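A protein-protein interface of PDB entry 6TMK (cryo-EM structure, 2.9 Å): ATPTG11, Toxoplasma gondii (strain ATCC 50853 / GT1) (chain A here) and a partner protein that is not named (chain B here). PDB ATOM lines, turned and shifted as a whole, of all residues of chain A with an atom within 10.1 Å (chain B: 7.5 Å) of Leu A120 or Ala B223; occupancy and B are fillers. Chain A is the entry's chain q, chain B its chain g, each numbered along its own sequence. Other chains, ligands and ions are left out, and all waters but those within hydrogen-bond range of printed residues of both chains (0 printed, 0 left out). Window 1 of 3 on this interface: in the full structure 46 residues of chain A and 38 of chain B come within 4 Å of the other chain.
The backbone carbonyl oxygen of Met A106 is in hydrogen-bond range of the guanidinium group of Arg B218 (3.3 Å). The backbone carbonyl oxygen (O) of Glu A112 lies within hydrogen-bond range of the side-chain amino group (NZ) of Lys B225, 3.1 Å away. O of Asp A114 is in hydrogen-bond range of NZ of Lys B225, at 2.4 Å. NE of Arg A116 lies within hydrogen-bond range of O of Leu B189. The side-chain amino group (NZ) of Lys B225 lies close to the backbone carbonyl oxygen (O) of Ala A111 (2.4 Å).
Hydrophobic or aromatic side chains of chain B within 4 Å of the printed part of chain A: Pro B185, Leu B189 and Leu B222. Along chain B the printed residues that touch a printed residue of chain A span positions 141 to 225. Of the 17 printed residues of chain A, 12 touch a printed residue of chain B. Hydrophobic or aromatic side chains of chain A that line the printed part of chain B: Met A106, Leu A108, Ala A111, Tyr A117, Leu A120 and Tyr A122. Along chain A the printed residues that touch a printed residue of chain B span positions 106 to 122.
Of the printed residues of chain B, Leu A120 touches Pro B185, Leu B189 and Ala B223. Of chain A, only Met A106, Ala A111, Asp A114, Arg A116 and Tyr A117 come within 4 Å of Leu B222. No residue of chain A comes within 4 Å of Asn B224. Printed residues of chain B within 4 Å of Asp A114: Leu B222 and Lys B225. Printed residues of chain B within 4 Å of Leu A108: Glu B217 (3.99 Å) and Arg B218 (3.5 Å). Printed residues of chain B within 4 Å of Ala A111: Lys B221, Leu B222 and Lys B225. Glu B226 touches none of the printed residues of chain A.
Among the printed residues, merely in contact across the chains: Glu A112 with Lys B221, Leu A120 with Pro B185, Tyr A122 with Glu B141, Arg A116 with Leu B222, Asp A114 with Leu B222, Leu A108 with Arg B218, Ala A111 with Leu B222, Tyr A117 with Leu B222, Asp A113 with Lys B225, Tyr A117 with Lys B225, Gln A119 with Leu B189, Tyr A117 with Ala B223, Ala A111 with Lys B221, Leu A120 with Ala B223, Met A106 with Leu B222, Gln A119 with Pro B185, Gln A121 with Pro B185, Tyr A122 with Asn B184, Leu A120 with Leu B189 and Leu A108 with Glu B217.
OD1 of Asp A114 is in salt-bridge range of NH1 of Arg A116 (2.7 Å). OH of Tyr A117 is in hydrogen-bond range of NZ of Lys A118 (2.7 Å). The side-chain amide oxygen (OD1) of Asn B184 lies close to the backbone NH (N) of Ala B186 (3.1 Å).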
ATOM      1  N   GLN A  25      33.568  14.200 -24.486  1.00  0.00           N
ATOM      2  CA  GLN A  25      34.031  14.726 -23.210  1.00  0.00           C
ATOM      3  C   GLN A  25      34.417  13.599 -22.264  1.00  0.00           C
ATOM      4  O   GLN A  25      35.373  13.728 -21.492  1.00  0.00           O
ATOM      5  CB  GLN A  25      32.953  15.604 -22.579  1.00  0.00           C
ATOM      6  CG  GLN A  25      32.393  16.675 -23.489  1.00  0.00           C
ATOM      7  CD  GLN A  25      33.458  17.589 -24.040  1.00  0.00           C
ATOM      8  OE1 GLN A  25      34.315  18.076 -23.306  1.00  0.00           O
ATOM      9  NE2 GLN A  25      33.404  17.839 -25.337  1.00  0.00           N
ATOM     10  N   MET A 106      34.040  19.440  -5.277  1.00  0.00           N
ATOM     11  CA  MET A 106      32.695  19.810  -5.696  1.00  0.00           C
ATOM     12  C   MET A 106      31.961  18.553  -6.133  1.00  0.00           C
ATOM     13  O   MET A 106      32.582  17.582  -6.574  1.00  0.00           O
ATOM     14  CB  MET A 106      32.736  20.831  -6.834  1.00  0.00           C
ATOM     15  CG  MET A 106      31.377  21.297  -7.289  1.00  0.00           C
ATOM     16  SD  MET A 106      31.485  22.641  -8.477  1.00  0.00           S
ATOM     17  CE  MET A 106      29.773  22.758  -8.963  1.00  0.00           C
ATOM     18  N   LEU A 108      28.315  16.674  -8.044  1.00  0.00           N
ATOM     19  CA  LEU A 108      27.408  16.811  -9.176  1.00  0.00           C
ATOM     20  C   LEU A 108      26.099  17.471  -8.774  1.00  0.00           C
ATOM     21  O   LEU A 108      25.458  18.130  -9.597  1.00  0.00           O
ATOM     22  CB  LEU A 108      27.133  15.442  -9.792  1.00  0.00           C
ATOM     23  CG  LEU A 108      28.356  14.655 -10.254  1.00  0.00           C
ATOM     24  CD1 LEU A 108      28.047  13.173 -10.277  1.00  0.00           C
ATOM     25  CD2 LEU A 108      28.805  15.125 -11.622  1.00  0.00           C
ATOM     26  N   GLN A 110      25.725  19.989  -6.577  1.00  0.00           N
ATOM     27  CA  GLN A 110      25.982  21.421  -6.674  1.00  0.00           C
ATOM     28  C   GLN A 110      26.139  21.846  -8.126  1.00  0.00           C
ATOM     29  O   GLN A 110      25.696  22.933  -8.517  1.00  0.00           O
ATOM     30  CB  GLN A 110      27.234  21.783  -5.881  1.00  0.00           C
ATOM     31  CG  GLN A 110      27.056  21.764  -4.379  1.00  0.00           C
ATOM     32  CD  GLN A 110      28.367  21.946  -3.644  1.00  0.00           C
ATOM     33  OE1 GLN A 110      28.712  21.160  -2.761  1.00  0.00           O
ATOM     34  NE2 GLN A 110      29.111  22.984  -4.008  1.00  0.00           N
ATOM     35  N   ALA A 111      26.773  21.001  -8.944  1.00  0.00           N
ATOM     36  CA  ALA A 111      26.941  21.335 -10.353  1.00  0.00           C
ATOM     37  C   ALA A 111      25.597  21.495 -11.053  1.00  0.00           C
ATOM     38  O   ALA A 111      25.435  22.367 -11.914  1.00  0.00           O
ATOM     39  CB  ALA A 111      27.773  20.260 -11.047  1.00  0.00           C
ATOM     40  N   GLU A 112      24.623  20.662 -10.695  1.00  0.00           N
ATOM     41  CA  GLU A 112      23.282  20.756 -11.262  1.00  0.00           C
ATOM     42  C   GLU A 112      22.443  21.851 -10.623  1.00  0.00           C
ATOM     43  O   GLU A 112      21.494  22.332 -11.250  1.00  0.00           O
ATOM     44  CB  GLU A 112      22.558  19.420 -11.120  1.00  0.00           C
ATOM     45  CG  GLU A 112      23.043  18.355 -12.083  1.00  0.00           C
ATOM     46  CD  GLU A 112      22.617  18.630 -13.513  1.00  0.00           C
ATOM     47  OE1 GLU A 112      23.432  18.403 -14.433  1.00  0.00           O
ATOM     48  OE2 GLU A 112      21.469  19.076 -13.718  1.00  0.00           O
ATOM     49  N   ASP A 113      22.764  22.251  -9.396  1.00  0.00           N
ATOM     50  CA  ASP A 113      22.001  23.282  -8.709  1.00  0.00           C
ATOM     51  C   ASP A 113      22.505  24.688  -8.994  1.00  0.00           C
ATOM     52  O   ASP A 113      21.776  25.653  -8.738  1.00  0.00           O
ATOM     53  CB  ASP A 113      22.033  23.038  -7.198  1.00  0.00           C
ATOM     54  CG  ASP A 113      21.330  21.757  -6.799  1.00  0.00           C
ATOM     55  OD1 ASP A 113      20.560  21.216  -7.620  1.00  0.00           O
ATOM     56  OD2 ASP A 113      21.549  21.286  -5.662  1.00  0.00           O
ATOM     57  N   ASP A 114      23.720  24.830  -9.513  1.00  0.00           N
ATOM     58  CA  ASP A 114      24.224  26.154  -9.840  1.00  0.00           C
ATOM     59  C   ASP A 114      23.404  26.773 -10.969  1.00  0.00           C
ATOM     60  O   ASP A 114      22.653  26.094 -11.674  1.00  0.00           O
ATOM     61  CB  ASP A 114      25.699  26.088 -10.234  1.00  0.00           C
ATOM     62  CG  ASP A 114      26.410  27.414 -10.055  1.00  0.00           C
ATOM     63  OD1 ASP A 114      27.654  27.440 -10.161  1.00  0.00           O
ATOM     64  OD2 ASP A 114      25.726  28.430  -9.812  1.00  0.00           O
ATOM     65  N   GLN A 115      23.557  28.089 -11.131  1.00  0.00           N
ATOM     66  CA  GLN A 115      22.753  28.863 -12.069  1.00  0.00           C
ATOM     67  C   GLN A 115      23.610  29.795 -12.917  1.00  0.00           C
ATOM     68  O   GLN A 115      23.098  30.779 -13.458  1.00  0.00           O
ATOM     69  CB  GLN A 115      21.686  29.665 -11.324  1.00  0.00           C
ATOM     70  CG  GLN A 115      20.621  28.806 -10.672  1.00  0.00           C
ATOM     71  CD  GLN A 115      19.681  28.182 -11.682  1.00  0.00           C
ATOM     72  OE1 GLN A 115      19.295  28.816 -12.663  1.00  0.00           O
ATOM     73  NE2 GLN A 115      19.313  26.930 -11.450  1.00  0.00           N
ATOM     74  N   ARG A 116      24.904  29.504 -13.046  1.00  0.00           N
ATOM     75  CA  ARG A 116      25.778  30.322 -13.872  1.00  0.00           C
ATOM     76  C   ARG A 116      25.523  30.118 -15.358  1.00  0.00           C
ATOM     77  O   ARG A 116      25.922  30.963 -16.166  1.00  0.00           O
ATOM     78  CB  ARG A 116      27.235  30.006 -13.543  1.00  0.00           C
ATOM     79  CG  ARG A 116      27.677  30.520 -12.190  1.00  0.00           C
ATOM     80  CD  ARG A 116      29.183  30.630 -12.110  1.00  0.00           C
ATOM     81  NE  ARG A 116      29.828  29.329 -12.270  1.00  0.00           N
ATOM     82  CZ  ARG A 116      30.156  28.525 -11.264  1.00  0.00           C
ATOM     83  NH1 ARG A 116      29.903  28.869 -10.012  1.00  0.00           N
ATOM     84  NH2 ARG A 116      30.736  27.366 -11.509  1.00  0.00           N
ATOM     85  N   TYR A 117      24.861  29.024 -15.733  1.00  0.00           N
ATOM     86  CA  TYR A 117      24.581  28.755 -17.138  1.00  0.00           C
ATOM     87  C   TYR A 117      23.685  29.813 -17.766  1.00  0.00           C
ATOM     88  O   TYR A 117      23.612  29.894 -18.997  1.00  0.00           O
ATOM     89  CB  TYR A 117      23.952  27.371 -17.283  1.00  0.00           C
ATOM     90  CG  TYR A 117      22.510  27.288 -16.848  1.00  0.00           C
ATOM     91  CD1 TYR A 117      22.155  27.462 -15.520  1.00  0.00           C
ATOM     92  CD2 TYR A 117      21.506  27.018 -17.763  1.00  0.00           C
ATOM     93  CE1 TYR A 117      20.839  27.381 -15.118  1.00  0.00           C
ATOM     94  CE2 TYR A 117      20.189  26.936 -17.372  1.00  0.00           C
ATOM     95  CZ  TYR A 117      19.861  27.117 -16.047  1.00  0.00           C
ATOM     96  OH  TYR A 117      18.548  27.037 -15.648  1.00  0.00           O
ATOM     97  N   LYS A 118      22.999  30.620 -16.957  1.00  0.00           N
ATOM     98  CA  LYS A 118      22.175  31.689 -17.508  1.00  0.00           C
ATOM     99  C   LYS A 118      23.017  32.761 -18.183  1.00  0.00           C
ATOM    100  O   LYS A 118      22.546  33.422 -19.114  1.00  0.00           O
ATOM    101  CB  LYS A 118      21.329  32.322 -16.406  1.00  0.00           C
ATOM    102  CG  LYS A 118      20.494  31.340 -15.615  1.00  0.00           C
ATOM    103  CD  LYS A 118      19.521  30.601 -16.501  1.00  0.00           C
ATOM    104  CE  LYS A 118      18.358  30.061 -15.701  1.00  0.00           C
ATOM    105  NZ  LYS A 118      17.411  29.289 -16.550  1.00  0.00           N
ATOM    106  N   GLN A 119      24.255  32.948 -17.731  1.00  0.00           N
ATOM    107  CA  GLN A 119      25.099  34.055 -18.154  1.00  0.00           C
ATOM    108  C   GLN A 119      26.118  33.638 -19.209  1.00  0.00           C
ATOM    109  O   GLN A 119      27.088  34.366 -19.447  1.00  0.00           O
ATOM    110  CB  GLN A 119      25.812  34.652 -16.943  1.00  0.00           C
ATOM    111  CG  GLN A 119      24.879  35.154 -15.861  1.00  0.00           C
ATOM    112  CD  GLN A 119      25.550  35.218 -14.506  1.00  0.00           C
ATOM    113  OE1 GLN A 119      26.766  35.384 -14.408  1.00  0.00           O
ATOM    114  NE2 GLN A 119      24.759  35.079 -13.448  1.00  0.00           N
ATOM    115  N   LEU A 120      25.915  32.490 -19.847  1.00  0.00           N
ATOM    116  CA  LEU A 120      26.873  31.940 -20.794  1.00  0.00           C
ATOM    117  C   LEU A 120      26.673  32.456 -22.213  1.00  0.00           C
ATOM    118  O   LEU A 120      27.278  31.919 -23.145  1.00  0.00           O
ATOM    119  CB  LEU A 120      26.785  30.415 -20.788  1.00  0.00           C
ATOM    120  CG  LEU A 120      27.638  29.671 -19.764  1.00  0.00           C
ATOM    121  CD1 LEU A 120      27.318  28.198 -19.815  1.00  0.00           C
ATOM    122  CD2 LEU A 120      29.108  29.888 -20.002  1.00  0.00           C
ATOM    123  N   GLN A 121      25.845  33.475 -22.400  1.00  0.00           N
ATOM    124  CA  GLN A 121      25.566  33.989 -23.731  1.00  0.00           C
ATOM    125  C   GLN A 121      26.739  34.809 -24.250  1.00  0.00           C
ATOM    126  O   GLN A 121      27.334  35.602 -23.516  1.00  0.00           O
ATOM    127  CB  GLN A 121      24.303  34.848 -23.714  1.00  0.00           C
ATOM    128  CG  GLN A 121      23.100  34.154 -23.114  1.00  0.00           C
ATOM    129  CD  GLN A 121      22.761  32.861 -23.827  1.00  0.00           C
ATOM    130  OE1 GLN A 121      23.109  32.669 -24.991  1.00  0.00           O
ATOM    131  NE2 GLN A 121      22.083  31.963 -23.126  1.00  0.00           N
ATOM    132  N   TYR A 122      27.072  34.610 -25.521  1.00  0.00           N
ATOM    133  CA  TYR A 122      28.103  35.422 -26.148  1.00  0.00           C
ATOM    134  C   TYR A 122      27.658  36.875 -26.227  1.00  0.00           C
ATOM    135  O   TYR A 122      26.473  37.181 -26.379  1.00  0.00           O
ATOM    136  CB  TYR A 122      28.415  34.909 -27.549  1.00  0.00           C
ATOM    137  CG  TYR A 122      29.556  33.929 -27.626  1.00  0.00           C
ATOM    138  CD1 TYR A 122      30.847  34.366 -27.852  1.00  0.00           C
ATOM    139  CD2 TYR A 122      29.344  32.569 -27.486  1.00  0.00           C
ATOM    140  CE1 TYR A 122      31.893  33.482 -27.930  1.00  0.00           C
ATOM    141  CE2 TYR A 122      30.389  31.679 -27.563  1.00  0.00           C
ATOM    142  CZ  TYR A 122      31.660  32.140 -27.785  1.00  0.00           C
ATOM    143  OH  TYR A 122      32.702  31.251 -27.861  1.00  0.00           O
ATOM    144  N   GLY A 123      28.626  37.778 -26.126  1.00  0.00           N
ATOM    145  CA  GLY A 123      28.333  39.193 -26.161  1.00  0.00           C
ATOM    146  C   GLY A 123      27.993  39.683 -27.551  1.00  0.00           C
ATOM    147  O   GLY A 123      27.488  38.926 -28.385  1.00  0.00           O
ATOM    148  N   GLU B 141      24.798  30.744 -32.703  1.00  0.00           N
ATOM    149  CA  GLU B 141      24.217  32.040 -32.382  1.00  0.00           C
ATOM    150  C   GLU B 141      25.241  33.163 -32.428  1.00  0.00           C
ATOM    151  O   GLU B 141      24.857  34.327 -32.577  1.00  0.00           O
ATOM    152  CB  GLU B 141      23.550  31.986 -31.006  1.00  0.00           C
ATOM    153  CG  GLU B 141      24.490  31.623 -29.846  1.00  0.00           C
ATOM    154  CD  GLU B 141      25.079  32.835 -29.143  1.00  0.00           C
ATOM    155  OE1 GLU B 141      24.573  33.959 -29.345  1.00  0.00           O
ATOM    156  OE2 GLU B 141      26.046  32.660 -28.372  1.00  0.00           O
ATOM    157  N   GLU B 183      34.900  37.281 -26.383  1.00  0.00           N
ATOM    158  CA  GLU B 183      35.524  36.272 -25.548  1.00  0.00           C
ATOM    159  C   GLU B 183      34.494  35.288 -25.015  1.00  0.00           C
ATOM    160  O   GLU B 183      33.325  35.623 -24.806  1.00  0.00           O
ATOM    161  CB  GLU B 183      36.262  36.933 -24.385  1.00  0.00           C
ATOM    162  CG  GLU B 183      37.224  36.015 -23.657  1.00  0.00           C
ATOM    163  CD  GLU B 183      37.886  36.686 -22.473  1.00  0.00           C
ATOM    164  OE1 GLU B 183      37.805  37.928 -22.369  1.00  0.00           O
ATOM    165  OE2 GLU B 183      38.487  35.973 -21.643  1.00  0.00           O
ATOM    166  N   ASN B 184      34.945  34.065 -24.799  1.00  0.00           N
ATOM    167  CA  ASN B 184      34.099  33.043 -24.210  1.00  0.00           C
ATOM    168  C   ASN B 184      33.751  33.428 -22.776  1.00  0.00           C
ATOM    169  O   ASN B 184      34.657  33.705 -21.981  1.00  0.00           O
ATOM    170  CB  ASN B 184      34.807  31.698 -24.244  1.00  0.00           C
ATOM    171  CG  ASN B 184      33.856  30.538 -24.128  1.00  0.00           C
ATOM    172  OD1 ASN B 184      32.756  30.670 -23.596  1.00  0.00           O
ATOM    173  ND2 ASN B 184      34.272  29.388 -24.630  1.00  0.00           N
ATOM    174  N   PRO B 185      32.469  33.463 -22.404  1.00  0.00           N
ATOM    175  CA  PRO B 185      32.128  33.760 -21.003  1.00  0.00           C
ATOM    176  C   PRO B 185      32.537  32.662 -20.044  1.00  0.00           C
ATOM    177  O   PRO B 185      32.612  32.910 -18.831  1.00  0.00           O
ATOM    178  CB  PRO B 185      30.604  33.920 -21.041  1.00  0.00           C
ATOM    179  CG  PRO B 185      30.183  33.154 -22.246  1.00  0.00           C
ATOM    180  CD  PRO B 185      31.266  33.333 -23.237  1.00  0.00           C
ATOM    181  N   ALA B 186      32.790  31.456 -20.549  1.00  0.00           N
ATOM    182  CA  ALA B 186      33.239  30.375 -19.687  1.00  0.00           C
ATOM    183  C   ALA B 186      34.580  30.701 -19.051  1.00  0.00           C
ATOM    184  O   ALA B 186      34.871  30.237 -17.946  1.00  0.00           O
ATOM    185  CB  ALA B 186      33.327  29.079 -20.484  1.00  0.00           C
ATOM    186  N   GLU B 187      35.404  31.503 -19.721  1.00  0.00           N
ATOM    187  CA  GLU B 187      36.712  31.831 -19.178  1.00  0.00           C
ATOM    188  C   GLU B 187      36.616  32.697 -17.931  1.00  0.00           C
ATOM    189  O   GLU B 187      37.559  32.718 -17.133  1.00  0.00           O
ATOM    190  CB  GLU B 187      37.551  32.533 -20.241  1.00  0.00           C
ATOM    191  CG  GLU B 187      37.863  31.656 -21.432  1.00  0.00           C
ATOM    192  CD  GLU B 187      38.732  32.348 -22.461  1.00  0.00           C
ATOM    193  OE1 GLU B 187      39.043  31.720 -23.495  1.00  0.00           O
ATOM    194  OE2 GLU B 187      39.105  33.519 -22.237  1.00  0.00           O
ATOM    195  N   LEU B 189      33.466  32.652 -16.008  1.00  0.00           N
ATOM    196  CA  LEU B 189      32.528  31.997 -15.104  1.00  0.00           C
ATOM    197  C   LEU B 189      33.069  30.696 -14.525  1.00  0.00           C
ATOM    198  O   LEU B 189      32.882  30.425 -13.335  1.00  0.00           O
ATOM    199  CB  LEU B 189      31.209  31.731 -15.824  1.00  0.00           C
ATOM    200  CG  LEU B 189      30.453  32.981 -16.267  1.00  0.00           C
ATOM    201  CD1 LEU B 189      29.254  32.598 -17.093  1.00  0.00           C
ATOM    202  CD2 LEU B 189      30.027  33.817 -15.079  1.00  0.00           C
ATOM    203  N   LEU B 190      33.737  29.886 -15.341  1.00  0.00           N
ATOM    204  CA  LEU B 190      34.275  28.586 -14.945  1.00  0.00           C
ATOM    205  C   LEU B 190      35.778  28.650 -14.723  1.00  0.00           C
ATOM    206  O   LEU B 190      36.518  27.730 -15.078  1.00  0.00           O
ATOM    207  CB  LEU B 190      33.930  27.539 -15.994  1.00  0.00           C
ATOM    208  CG  LEU B 190      32.483  27.052 -16.011  1.00  0.00           C
ATOM    209  CD1 LEU B 190      31.530  28.177 -16.323  1.00  0.00           C
ATOM    210  CD2 LEU B 190      32.330  25.954 -17.029  1.00  0.00           C
ATOM    211  N   GLU B 217      33.580  16.506 -16.074  1.00  0.00           N
ATOM    212  CA  GLU B 217      32.159  16.248 -15.891  1.00  0.00           C
ATOM    213  C   GLU B 217      31.509  17.345 -15.064  1.00  0.00           C
ATOM    214  O   GLU B 217      30.371  17.742 -15.335  1.00  0.00           O
ATOM    215  CB  GLU B 217      31.959  14.887 -15.234  1.00  0.00           C
ATOM    216  CG  GLU B 217      30.516  14.454 -15.161  1.00  0.00           C
ATOM    217  CD  GLU B 217      30.362  12.952 -15.045  1.00  0.00           C
ATOM    218  OE1 GLU B 217      31.334  12.285 -14.634  1.00  0.00           O
ATOM    219  OE2 GLU B 217      29.270  12.439 -15.363  1.00  0.00           O
ATOM    220  N   ARG B 218      32.217  17.854 -14.055  1.00  0.00           N
ATOM    221  CA  ARG B 218      31.678  18.972 -13.289  1.00  0.00           C
ATOM    222  C   ARG B 218      31.455  20.179 -14.191  1.00  0.00           C
ATOM    223  O   ARG B 218      30.397  20.821 -14.148  1.00  0.00           O
ATOM    224  CB  ARG B 218      32.625  19.328 -12.143  1.00  0.00           C
ATOM    225  CG  ARG B 218      32.775  18.275 -11.041  1.00  0.00           C
ATOM    226  CD  ARG B 218      31.450  17.711 -10.567  1.00  0.00           C
ATOM    227  NE  ARG B 218      31.619  16.624  -9.608  1.00  0.00           N
ATOM    228  CZ  ARG B 218      32.014  15.398  -9.930  1.00  0.00           C
ATOM    229  NH1 ARG B 218      32.307  15.097 -11.184  1.00  0.00           N
ATOM    230  NH2 ARG B 218      32.130  14.475  -8.992  1.00  0.00           N
ATOM    231  N   MET B 219      32.440  20.488 -15.036  1.00  0.00           N
ATOM    232  CA  MET B 219      32.297  21.601 -15.971  1.00  0.00           C
ATOM    233  C   MET B 219      31.135  21.376 -16.929  1.00  0.00           C
ATOM    234  O   MET B 219      30.341  22.289 -17.186  1.00  0.00           O
ATOM    235  CB  MET B 219      33.590  21.775 -16.757  1.00  0.00           C
ATOM    236  CG  MET B 219      34.775  22.188 -15.928  1.00  0.00           C
ATOM    237  SD  MET B 219      36.312  21.974 -16.831  1.00  0.00           S
ATOM    238  CE  MET B 219      36.223  23.373 -17.931  1.00  0.00           C
ATOM    239  N   TYR B 220      31.026  20.164 -17.472  1.00  0.00           N
ATOM    240  CA  TYR B 220      29.970  19.874 -18.433  1.00  0.00           C
ATOM    241  C   TYR B 220      28.598  20.034 -17.800  1.00  0.00           C
ATOM    242  O   TYR B 220      27.693  20.619 -18.403  1.00  0.00           O
ATOM    243  CB  TYR B 220      30.151  18.462 -18.980  1.00  0.00           C
ATOM    244  CG  TYR B 220      29.116  18.043 -19.990  1.00  0.00           C
ATOM    245  CD1 TYR B 220      29.152  18.524 -21.287  1.00  0.00           C
ATOM    246  CD2 TYR B 220      28.107  17.161 -19.649  1.00  0.00           C
ATOM    247  CE1 TYR B 220      28.209  18.143 -22.213  1.00  0.00           C
ATOM    248  CE2 TYR B 220      27.160  16.775 -20.568  1.00  0.00           C
ATOM    249  CZ  TYR B 220      27.216  17.268 -21.849  1.00  0.00           C
ATOM    250  OH  TYR B 220      26.272  16.881 -22.768  1.00  0.00           O
ATOM    251  N   LYS B 221      28.423  19.515 -16.584  1.00  0.00           N
ATOM    252  CA  LYS B 221      27.146  19.662 -15.902  1.00  0.00           C
ATOM    253  C   LYS B 221      26.835  21.128 -15.647  1.00  0.00           C
ATOM    254  O   LYS B 221      25.730  21.604 -15.944  1.00  0.00           O
ATOM    255  CB  LYS B 221      27.170  18.887 -14.588  1.00  0.00           C
ATOM    256  CG  LYS B 221      27.237  17.387 -14.756  1.00  0.00           C
ATOM    257  CD  LYS B 221      25.887  16.806 -15.109  1.00  0.00           C
ATOM    258  CE  LYS B 221      26.019  15.471 -15.816  1.00  0.00           C
ATOM    259  NZ  LYS B 221      24.848  15.189 -16.690  1.00  0.00           N
ATOM    260  N   LEU B 222      27.814  21.869 -15.120  1.00  0.00           N
ATOM    261  CA  LEU B 222      27.612  23.287 -14.852  1.00  0.00           C
ATOM    262  C   LEU B 222      27.179  24.037 -16.101  1.00  0.00           C
ATOM    263  O   LEU B 222      26.326  24.929 -16.035  1.00  0.00           O
ATOM    264  CB  LEU B 222      28.896  23.895 -14.299  1.00  0.00           C
ATOM    265  CG  LEU B 222      29.141  23.762 -12.803  1.00  0.00           C
ATOM    266  CD1 LEU B 222      30.565  24.138 -12.498  1.00  0.00           C
ATOM    267  CD2 LEU B 222      28.182  24.634 -12.025  1.00  0.00           C
ATOM    268  N   ALA B 223      27.757  23.694 -17.248  1.00  0.00           N
ATOM    269  CA  ALA B 223      27.456  24.437 -18.464  1.00  0.00           C
ATOM    270  C   ALA B 223      26.144  24.006 -19.099  1.00  0.00           C
ATOM    271  O   ALA B 223      25.451  24.835 -19.695  1.00  0.00           O
ATOM    272  CB  ALA B 223      28.592  24.275 -19.470  1.00  0.00           C
ATOM    273  N   ASN B 224      25.787  22.730 -18.989  1.00  0.00           N
ATOM    274  CA  ASN B 224      24.676  22.175 -19.748  1.00  0.00           C
ATOM    275  C   ASN B 224      23.373  22.118 -18.964  1.00  0.00           C
ATOM    276  O   ASN B 224      22.336  22.562 -19.465  1.00  0.00           O
ATOM    277  CB  ASN B 224      25.048  20.779 -20.246  1.00  0.00           C
ATOM    278  CG  ASN B 224      26.098  20.819 -21.330  1.00  0.00           C
ATOM    279  OD1 ASN B 224      27.294  20.865 -21.052  1.00  0.00           O
ATOM    280  ND2 ASN B 224      25.653  20.822 -22.576  1.00  0.00           N
ATOM    281  N   LYS B 225      23.393  21.577 -17.745  1.00  0.00           N
ATOM    282  CA  LYS B 225      22.179  21.451 -16.941  1.00  0.00           C
ATOM    283  C   LYS B 225      21.135  20.610 -17.677  1.00  0.00           C
ATOM    284  O   LYS B 225      20.060  21.083 -18.051  1.00  0.00           O
ATOM    285  CB  LYS B 225      21.607  22.827 -16.586  1.00  0.00           C
ATOM    286  CG  LYS B 225      22.589  23.774 -15.939  1.00  0.00           C
ATOM    287  CD  LYS B 225      23.040  23.255 -14.595  1.00  0.00           C
ATOM    288  CE  LYS B 225      23.822  24.304 -13.835  1.00  0.00           C
ATOM    289  NZ  LYS B 225      23.805  24.052 -12.371  1.00  0.00           N
ATOM    290  N   GLU B 226      21.482  19.345 -17.886  1.00  0.00           N
ATOM    291  CA  GLU B 226      20.594  18.404 -18.560  1.00  0.00           C
ATOM    292  C   GLU B 226      20.229  18.905 -19.953  1.00  0.00           C
ATOM    293  O   GLU B 226      20.843  19.838 -20.468  1.00  0.00           O
ATOM    294  CB  GLU B 226      19.329  18.174 -17.732  1.00  0.00           C
ATOM    295  CG  GLU B 226      18.312  17.272 -18.399  1.00  0.00           C
ATOM    296  CD  GLU B 226      17.219  18.049 -19.106  1.00  0.00           C
ATOM    297  OE1 GLU B 226      16.608  18.933 -18.470  1.00  0.00           O
ATOM    298  OE2 GLU B 226      16.967  17.775 -20.298  1.00  0.00           O
